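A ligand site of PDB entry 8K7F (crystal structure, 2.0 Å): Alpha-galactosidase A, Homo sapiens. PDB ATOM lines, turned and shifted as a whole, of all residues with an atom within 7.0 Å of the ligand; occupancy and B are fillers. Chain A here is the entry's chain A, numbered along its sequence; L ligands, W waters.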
ATOM      1  N   LEU A  14     -22.232  23.303 -30.006  1.00  0.00           N
ATOM      2  CA  LEU A  14     -20.785  23.278 -29.823  1.00  0.00           C
ATOM      3  C   LEU A  14     -20.159  22.919 -31.162  1.00  0.00           C
ATOM      4  O   LEU A  14     -20.628  22.001 -31.832  1.00  0.00           O
ATOM      5  CB  LEU A  14     -20.420  22.247 -28.742  1.00  0.00           C
ATOM      6  CG  LEU A  14     -18.975  21.987 -28.333  1.00  0.00           C
ATOM      7  CD1 LEU A  14     -18.309  23.275 -27.866  1.00  0.00           C
ATOM      8  CD2 LEU A  14     -18.967  20.949 -27.200  1.00  0.00           C
ATOM      9  N   TRP A  16     -17.301  21.597 -32.250  1.00  0.00           N
ATOM     10  CA  TRP A  16     -16.130  20.734 -32.458  1.00  0.00           C
ATOM     11  C   TRP A  16     -16.357  19.626 -33.480  1.00  0.00           C
ATOM     12  O   TRP A  16     -15.571  19.465 -34.420  1.00  0.00           O
ATOM     13  CB  TRP A  16     -15.670  20.121 -31.144  1.00  0.00           C
ATOM     14  CG  TRP A  16     -14.421  19.340 -31.381  1.00  0.00           C
ATOM     15  CD1 TRP A  16     -14.266  17.990 -31.327  1.00  0.00           C
ATOM     16  CD2 TRP A  16     -13.139  19.879 -31.768  1.00  0.00           C
ATOM     17  NE1 TRP A  16     -12.969  17.648 -31.617  1.00  0.00           N
ATOM     18  CE2 TRP A  16     -12.254  18.787 -31.898  1.00  0.00           C
ATOM     19  CE3 TRP A  16     -12.658  21.169 -31.990  1.00  0.00           C
ATOM     20  CZ2 TRP A  16     -10.912  18.942 -32.254  1.00  0.00           C
ATOM     21  CZ3 TRP A  16     -11.307  21.330 -32.355  1.00  0.00           C
ATOM     22  CH2 TRP A  16     -10.465  20.222 -32.482  1.00  0.00           C
ATOM     23  N   CYS A  21     -10.980  21.890 -36.194  1.00  0.00           N
ATOM     24  CA  CYS A  21      -9.993  22.960 -36.062  1.00  0.00           C
ATOM     25  C   CYS A  21      -9.667  23.530 -37.423  1.00  0.00           C
ATOM     26  O   CYS A  21      -8.498  23.585 -37.818  1.00  0.00           O
ATOM     27  CB  CYS A  21      -8.731  22.427 -35.380  1.00  0.00           C
ATOM     28  SG  CYS A  21      -7.570  23.724 -34.857  1.00  0.00           S
ATOM     29  N   ASP A  61     -15.399  25.802 -29.130  1.00  0.00           N
ATOM     30  CA  ASP A  61     -14.488  24.763 -28.666  1.00  0.00           C
ATOM     31  C   ASP A  61     -13.046  25.220 -28.955  1.00  0.00           C
ATOM     32  O   ASP A  61     -12.776  26.425 -29.052  1.00  0.00           O
ATOM     33  CB  ASP A  61     -14.862  23.420 -29.318  1.00  0.00           C
ATOM     34  CG  ASP A  61     -14.433  22.216 -28.461  1.00  0.00           C
ATOM     35  OD1 ASP A  61     -13.234  21.908 -28.445  1.00  0.00           O
ATOM     36  OD2 ASP A  61     -15.290  21.611 -27.774  1.00  0.00           O
ATOM     37  N   ASP A  62     -12.130  24.273 -29.077  1.00  0.00           N
ATOM     38  CA  ASP A  62     -10.708  24.592 -29.282  1.00  0.00           C
ATOM     39  C   ASP A  62     -10.510  25.333 -30.615  1.00  0.00           C
ATOM     40  O   ASP A  62     -11.371  25.312 -31.497  1.00  0.00           O
ATOM     41  CB  ASP A  62      -9.910  23.292 -29.246  1.00  0.00           C
ATOM     42  CG  ASP A  62      -8.419  23.490 -28.932  1.00  0.00           C
ATOM     43  OD1 ASP A  62      -7.921  24.628 -28.878  1.00  0.00           O
ATOM     44  OD2 ASP A  62      -7.754  22.454 -28.731  1.00  0.00           O
ATOM     45  N   CYS A  63      -9.367  26.022 -30.719  1.00  0.00           N
ATOM     46  CA  CYS A  63      -8.890  26.733 -31.915  1.00  0.00           C
ATOM     47  C   CYS A  63      -9.527  28.112 -32.106  1.00  0.00           C
ATOM     48  O   CYS A  63      -9.708  28.548 -33.254  1.00  0.00           O
ATOM     49  CB  CYS A  63      -9.076  25.883 -33.186  1.00  0.00           C
ATOM     50  SG  CYS A  63      -8.265  24.252 -33.009  1.00  0.00           S
ATOM     51  N   TYR A 103     -13.667  27.681 -24.390  1.00  0.00           N
ATOM     52  CA  TYR A 103     -12.865  26.499 -24.166  1.00  0.00           C
ATOM     53  C   TYR A 103     -11.487  26.901 -23.649  1.00  0.00           C
ATOM     54  O   TYR A 103     -10.915  27.892 -24.104  1.00  0.00           O
ATOM     55  CB  TYR A 103     -12.733  25.688 -25.488  1.00  0.00           C
ATOM     56  CG  TYR A 103     -11.645  24.624 -25.519  1.00  0.00           C
ATOM     57  CD1 TYR A 103     -10.308  24.959 -25.701  1.00  0.00           C
ATOM     58  CD2 TYR A 103     -11.971  23.267 -25.406  1.00  0.00           C
ATOM     59  CE1 TYR A 103      -9.314  23.988 -25.734  1.00  0.00           C
ATOM     60  CE2 TYR A 103     -10.974  22.281 -25.448  1.00  0.00           C
ATOM     61  CZ  TYR A 103      -9.652  22.653 -25.604  1.00  0.00           C
ATOM     62  OH  TYR A 103      -8.657  21.695 -25.648  1.00  0.00           O
ATOM     63  N   ASP A 105      -7.804  24.830 -21.437  1.00  0.00           N
ATOM     64  CA  ASP A 105      -7.171  23.567 -21.089  1.00  0.00           C
ATOM     65  C   ASP A 105      -6.425  23.685 -19.764  1.00  0.00           C
ATOM     66  O   ASP A 105      -5.759  24.683 -19.508  1.00  0.00           O
ATOM     67  CB  ASP A 105      -6.232  23.128 -22.220  1.00  0.00           C
ATOM     68  CG  ASP A 105      -5.790  21.673 -22.114  1.00  0.00           C
ATOM     69  OD1 ASP A 105      -5.026  21.349 -21.183  1.00  0.00           O
ATOM     70  OD2 ASP A 105      -6.213  20.855 -22.953  1.00  0.00           O
ATOM     71  N   THR A 110      -3.485  23.637 -25.173  1.00  0.00           N
ATOM     72  CA  THR A 110      -4.730  22.984 -25.529  1.00  0.00           C
ATOM     73  C   THR A 110      -4.423  21.759 -26.389  1.00  0.00           C
ATOM     74  O   THR A 110      -3.311  21.585 -26.877  1.00  0.00           O
ATOM     75  CB  THR A 110      -5.686  23.910 -26.272  1.00  0.00           C
ATOM     76  OG1 THR A 110      -5.237  24.071 -27.620  1.00  0.00           O
ATOM     77  CG2 THR A 110      -5.791  25.273 -25.583  1.00  0.00           C
ATOM     78  N   CYS A 111      -5.428  20.907 -26.556  1.00  0.00           N
ATOM     79  CA  CYS A 111      -5.212  19.681 -27.322  1.00  0.00           C
ATOM     80  C   CYS A 111      -4.772  19.979 -28.750  1.00  0.00           C
ATOM     81  O   CYS A 111      -4.018  19.184 -29.338  1.00  0.00           O
ATOM     82  CB  CYS A 111      -6.473  18.815 -27.314  1.00  0.00           C
ATOM     83  SG  CYS A 111      -6.848  18.100 -25.711  1.00  0.00           S
ATOM     84  N   ALA A 112      -5.198  21.093 -29.326  1.00  0.00           N
ATOM     85  CA  ALA A 112      -4.779  21.464 -30.679  1.00  0.00           C
ATOM     86  C   ALA A 112      -3.480  22.275 -30.708  1.00  0.00           C
ATOM     87  O   ALA A 112      -2.999  22.603 -31.802  1.00  0.00           O
ATOM     88  CB  ALA A 112      -5.886  22.263 -31.374  1.00  0.00           C
ATOM     89  N   GLY A 113      -2.907  22.612 -29.550  1.00  0.00           N
ATOM     90  CA  GLY A 113      -1.593  23.239 -29.465  1.00  0.00           C
ATOM     91  C   GLY A 113      -1.562  24.707 -29.070  1.00  0.00           C
ATOM     92  O   GLY A 113      -0.490  25.317 -29.113  1.00  0.00           O
ATOM     93  N   LYS A 137     -15.730  25.074 -21.079  1.00  0.00           N
ATOM     94  CA  LYS A 137     -15.300  23.692 -21.275  1.00  0.00           C
ATOM     95  C   LYS A 137     -13.797  23.625 -21.027  1.00  0.00           C
ATOM     96  O   LYS A 137     -13.021  24.311 -21.703  1.00  0.00           O
ATOM     97  CB  LYS A 137     -15.634  23.193 -22.674  1.00  0.00           C
ATOM     98  CG  LYS A 137     -15.229  21.735 -22.932  1.00  0.00           C
ATOM     99  CD  LYS A 137     -15.624  21.288 -24.335  1.00  0.00           C
ATOM    100  CE  LYS A 137     -14.861  20.035 -24.778  1.00  0.00           C
ATOM    101  NZ  LYS A 137     -15.347  19.510 -26.083  1.00  0.00           N
ATOM    102  N   ASP A 139     -10.535  21.401 -20.952  1.00  0.00           N
ATOM    103  CA  ASP A 139      -9.919  20.190 -21.477  1.00  0.00           C
ATOM    104  C   ASP A 139      -8.728  19.762 -20.620  1.00  0.00           C
ATOM    105  O   ASP A 139      -8.223  20.523 -19.772  1.00  0.00           O
ATOM    106  CB  ASP A 139      -9.492  20.421 -22.924  1.00  0.00           C
ATOM    107  CG  ASP A 139      -9.518  19.160 -23.767  1.00  0.00           C
ATOM    108  OD1 ASP A 139      -9.594  18.039 -23.207  1.00  0.00           O
ATOM    109  OD2 ASP A 139      -9.458  19.295 -24.996  1.00  0.00           O
ATOM    110  N   GLY A 140      -8.237  18.545 -20.863  1.00  0.00           N
ATOM    111  CA  GLY A 140      -7.165  18.023 -20.025  1.00  0.00           C
ATOM    112  C   GLY A 140      -5.861  17.602 -20.697  1.00  0.00           C
ATOM    113  O   GLY A 140      -5.113  16.807 -20.124  1.00  0.00           O
ATOM    114  N   CYS A 141      -5.558  18.131 -21.888  1.00  0.00           N
ATOM    115  CA  CYS A 141      -4.315  17.762 -22.564  1.00  0.00           C
ATOM    116  C   CYS A 141      -3.098  18.417 -21.917  1.00  0.00           C
ATOM    117  O   CYS A 141      -3.205  19.440 -21.223  1.00  0.00           O
ATOM    118  CB  CYS A 141      -4.345  18.174 -24.039  1.00  0.00           C
ATOM    119  SG  CYS A 141      -5.191  17.048 -25.141  1.00  0.00           S
ATOM    120  N   GLU A 172     -13.280  17.746 -18.245  1.00  0.00           N
ATOM    121  CA  GLU A 172     -12.890  16.472 -18.842  1.00  0.00           C
ATOM    122  C   GLU A 172     -12.052  15.621 -17.891  1.00  0.00           C
ATOM    123  O   GLU A 172     -11.460  14.614 -18.298  1.00  0.00           O
ATOM    124  CB  GLU A 172     -12.168  16.702 -20.170  1.00  0.00           C
ATOM    125  CG  GLU A 172     -13.068  17.402 -21.187  1.00  0.00           C
ATOM    126  CD  GLU A 172     -12.714  17.089 -22.632  1.00  0.00           C
ATOM    127  OE1 GLU A 172     -12.401  15.912 -22.943  1.00  0.00           O
ATOM    128  OE2 GLU A 172     -12.765  18.021 -23.463  1.00  0.00           O
ATOM    129  N   LEU A 175     -12.343  11.617 -17.797  1.00  0.00           N
ATOM    130  CA  LEU A 175     -11.815  11.038 -19.022  1.00  0.00           C
ATOM    131  C   LEU A 175     -10.287  10.923 -18.992  1.00  0.00           C
ATOM    132  O   LEU A 175      -9.731   9.888 -19.353  1.00  0.00           O
ATOM    133  CB  LEU A 175     -12.254  11.908 -20.212  1.00  0.00           C
ATOM    134  CG  LEU A 175     -11.600  11.551 -21.545  1.00  0.00           C
ATOM    135  CD1 LEU A 175     -11.984  10.130 -21.930  1.00  0.00           C
ATOM    136  CD2 LEU A 175     -11.989  12.559 -22.609  1.00  0.00           C
ATOM    137  N   TYR A 176      -9.606  11.977 -18.541  1.00  0.00           N
ATOM    138  CA  TYR A 176      -8.147  11.949 -18.529  1.00  0.00           C
ATOM    139  C   TYR A 176      -7.586  11.187 -17.341  1.00  0.00           C
ATOM    140  O   TYR A 176      -6.421  10.781 -17.368  1.00  0.00           O
ATOM    141  CB  TYR A 176      -7.582  13.379 -18.527  1.00  0.00           C
ATOM    142  CG  TYR A 176      -7.703  14.012 -19.887  1.00  0.00           C
ATOM    143  CD1 TYR A 176      -8.872  14.654 -20.270  1.00  0.00           C
ATOM    144  CD2 TYR A 176      -6.648  13.949 -20.799  1.00  0.00           C
ATOM    145  CE1 TYR A 176      -8.995  15.223 -21.516  1.00  0.00           C
ATOM    146  CE2 TYR A 176      -6.768  14.531 -22.065  1.00  0.00           C
ATOM    147  CZ  TYR A 176      -7.944  15.161 -22.408  1.00  0.00           C
ATOM    148  OH  TYR A 176      -8.068  15.744 -23.654  1.00  0.00           O
ATOM    149  N   ARG A 196     -16.960  14.900 -18.771  1.00  0.00           N
ATOM    150  CA  ARG A 196     -16.781  13.925 -19.821  1.00  0.00           C
ATOM    151  C   ARG A 196     -16.166  12.652 -19.262  1.00  0.00           C
ATOM    152  O   ARG A 196     -15.158  12.700 -18.556  1.00  0.00           O
ATOM    153  CB  ARG A 196     -15.906  14.513 -20.932  1.00  0.00           C
ATOM    154  CG  ARG A 196     -16.627  15.545 -21.818  1.00  0.00           C
ATOM    155  CD  ARG A 196     -17.416  14.829 -22.897  1.00  0.00           C
ATOM    156  NE  ARG A 196     -16.576  13.824 -23.541  1.00  0.00           N
ATOM    157  CZ  ARG A 196     -15.684  14.075 -24.490  1.00  0.00           C
ATOM    158  NH1 ARG A 196     -15.533  15.297 -24.988  1.00  0.00           N
ATOM    159  NH2 ARG A 196     -14.901  13.093 -24.921  1.00  0.00           N
ATOM    160  N   PHE A 198     -15.769   9.552 -21.391  1.00  0.00           N
ATOM    161  CA  PHE A 198     -15.396   8.564 -22.393  1.00  0.00           C
ATOM    162  C   PHE A 198     -14.878   9.261 -23.641  1.00  0.00           C
ATOM    163  O   PHE A 198     -15.002  10.478 -23.805  1.00  0.00           O
ATOM    164  CB  PHE A 198     -16.592   7.654 -22.707  1.00  0.00           C
ATOM    165  CG  PHE A 198     -16.251   6.467 -23.572  1.00  0.00           C
ATOM    166  CD1 PHE A 198     -15.420   5.457 -23.116  1.00  0.00           C
ATOM    167  CD2 PHE A 198     -16.746   6.396 -24.870  1.00  0.00           C
ATOM    168  CE1 PHE A 198     -15.091   4.379 -23.927  1.00  0.00           C
ATOM    169  CE2 PHE A 198     -16.417   5.317 -25.682  1.00  0.00           C
ATOM    170  CZ  PHE A 198     -15.590   4.309 -25.206  1.00  0.00           C
ATOM    171  N   ALA A 199     -14.313   8.455 -24.552  1.00  0.00           N
ATOM    172  CA  ALA A 199     -13.678   8.956 -25.767  1.00  0.00           C
ATOM    173  C   ALA A 199     -14.616   9.836 -26.586  1.00  0.00           C
ATOM    174  O   ALA A 199     -15.839   9.648 -26.572  1.00  0.00           O
ATOM    175  CB  ALA A 199     -13.209   7.778 -26.629  1.00  0.00           C
ATOM    176  N   ASP A 200     -14.021  10.798 -27.301  1.00  0.00           N
ATOM    177  CA  ASP A 200     -14.770  11.732 -28.146  1.00  0.00           C
ATOM    178  C   ASP A 200     -15.699  10.986 -29.089  1.00  0.00           C
ATOM    179  O   ASP A 200     -15.350   9.939 -29.643  1.00  0.00           O
ATOM    180  CB  ASP A 200     -13.823  12.583 -28.990  1.00  0.00           C
ATOM    181  CG  ASP A 200     -12.878  13.435 -28.172  1.00  0.00           C
ATOM    182  OD1 ASP A 200     -12.947  13.423 -26.910  1.00  0.00           O
ATOM    183  OD2 ASP A 200     -12.039  14.128 -28.806  1.00  0.00           O
ATOM    184  N   ILE A 201     -16.873  11.561 -29.306  1.00  0.00           N
ATOM    185  CA  ILE A 201     -17.822  11.032 -30.273  1.00  0.00           C
ATOM    186  C   ILE A 201     -17.364  11.403 -31.681  1.00  0.00           C
ATOM    187  O   ILE A 201     -16.694  12.429 -31.904  1.00  0.00           O
ATOM    188  CB  ILE A 201     -19.238  11.579 -29.976  1.00  0.00           C
ATOM    189  CG1 ILE A 201     -20.300  10.779 -30.728  1.00  0.00           C
ATOM    190  CG2 ILE A 201     -19.326  13.065 -30.320  1.00  0.00           C
ATOM    191  CD1 ILE A 201     -21.693  10.988 -30.186  1.00  0.00           C
ATOM    192  N   ASP A 235     -20.860  13.259 -24.428  1.00  0.00           N
ATOM    193  CA  ASP A 235     -20.455  14.030 -25.610  1.00  0.00           C
ATOM    194  C   ASP A 235     -21.617  14.427 -26.530  1.00  0.00           C
ATOM    195  O   ASP A 235     -22.783  14.145 -26.246  1.00  0.00           O
ATOM    196  CB  ASP A 235     -19.356  13.296 -26.399  1.00  0.00           C
ATOM    197  CG  ASP A 235     -18.323  14.268 -26.987  1.00  0.00           C
ATOM    198  OD1 ASP A 235     -18.508  15.500 -26.838  1.00  0.00           O
ATOM    199  OD2 ASP A 235     -17.337  13.793 -27.597  1.00  0.00           O
ATOM    200  N   MET A 236     -21.273  15.145 -27.599  1.00  0.00           N
ATOM    201  CA  MET A 236     -22.235  15.911 -28.397  1.00  0.00           C
ATOM    202  C   MET A 236     -23.236  15.031 -29.133  1.00  0.00           C
ATOM    203  O   MET A 236     -22.974  13.871 -29.454  1.00  0.00           O
ATOM    204  CB  MET A 236     -21.502  16.793 -29.417  1.00  0.00           C
ATOM    205  CG  MET A 236     -20.464  17.738 -28.820  1.00  0.00           C
ATOM    206  SD  MET A 236     -19.244  18.284 -30.055  1.00  0.00           S
ATOM    207  CE  MET A 236     -18.049  16.962 -29.899  1.00  0.00           C
HETATM  208  C1  LIG L   1     -10.893  18.608 -28.469  1.00  0.00           C
HETATM  209  C2  LIG L   1     -12.398  18.564 -28.212  1.00  0.00           C
HETATM  210  C3  LIG L   1     -10.429  20.040 -28.661  1.00  0.00           C
HETATM  211  C4  LIG L   1     -12.466  17.210 -27.528  1.00  0.00           C
HETATM  212  C5  LIG L   1     -11.320  17.328 -26.512  1.00  0.00           C
HETATM  213  C6  LIG L   1     -10.759  15.963 -26.122  1.00  0.00           C
HETATM  214  N1  LIG L   1     -10.274  18.080 -27.230  1.00  0.00           N
HETATM  215  O1  LIG L   1     -12.765  19.610 -27.304  1.00  0.00           O
HETATM  216  O2  LIG L   1     -13.733  17.022 -26.870  1.00  0.00           O
HETATM  217  O3  LIG L   1      -9.012  20.028 -28.923  1.00  0.00           O
HETATM  218  O4  LIG L   1     -11.749  15.207 -25.434  1.00  0.00           O
HETATM  219  O   HOH W   1     -15.548  15.473 -28.581  1.00  0.00           O
HETATM  220  O   HOH W   2      -7.566  18.512 -30.698  1.00  0.00           O
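OD1 of Asp 200 sits at hydrogen-bond distance from O4 of the ligand, 2.6 Å away. The side-chain carboxylate of Asp 61 sits at hydrogen-bond distance from an oxygen (O1) of the ligand, 2.6 Å away. An oxygen (O4) of the ligand sits at hydrogen-bond distance from the side-chain carboxylate (OE1) of Glu 172 (2.7 Å). A nitrogen (N1) of the ligand lies within salt-bridge range of the side-chain carboxylate (OD2) of Asp 139 (2.7 Å). The side-chain carboxylate (OD2) of Asp 62 lies within hydrogen-bond range of an oxygen (O3) of the ligand, at 2.7 Å. An oxygen (O1) of the ligand lies within hydrogen-bond range of the side-chain amino group (NZ) of Lys 137 (2.9 Å). O2 of the ligand sits at hydrogen-bond distance from NH1 of Arg 196. SG of Cys 111 sits at hydrogen-bond distance from N1 of the ligand (3.7 Å).
The side-chain carboxylate (OD2) of Asp 61 is in salt-bridge range of the side-chain amino group (NZ) of Lys 137, 2.7 Å away. The side-chain carboxylate (OD2) of Asp 62 lies within hydrogen-bond range of the side-chain hydroxyl (OH) of Tyr 103 (3.3 Å). The backbone carbonyl oxygen (O) of Arg 196 is in hydrogen-bond range of the backbone NH (N) of Leu 175, at 3.1 Å. The guanidinium group (NH2) of Arg 196 lies within hydrogen-bond range of the backbone carbonyl oxygen (O) of Phe 198 (2.8 Å). The side-chain hydroxyl (OH) of Tyr 176 lies within hydrogen-bond range of the side-chain sulfur (SG) of Cys 111 (3.4 Å). The side-chain sulfur (SG) of Cys 111 forms a disulfide with the side-chain sulfur (SG) of Cys 141. The side-chain sulfur (SG) of Cys 141 lies within hydrogen-bond range of the side-chain hydroxyl (OH) of Tyr 176, 3.5 Å away. N of Ala 112 lies close to OG1 of Thr 110 (3.4 Å).
Water W1 bridges the side-chain carboxylate (OD2) of Asp 235 and an oxygen (O2) of the ligand.
Merely in contact with the ligand: Trp 16 (3.6 Å), Tyr 103 (3.7 Å), Ala 112 (3.98 Å), Leu 175 (3.9 Å) and Tyr 176 (3.7 Å). Hydrophobic or aromatic side chains that line the ligand: Trp 16, Tyr 103 and Leu 175. Of the 26 residues printed, 13 come within 4 Å of the ligand. The nearest printed residue that does not touch the ligand is Asp 235 (4.9 Å).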
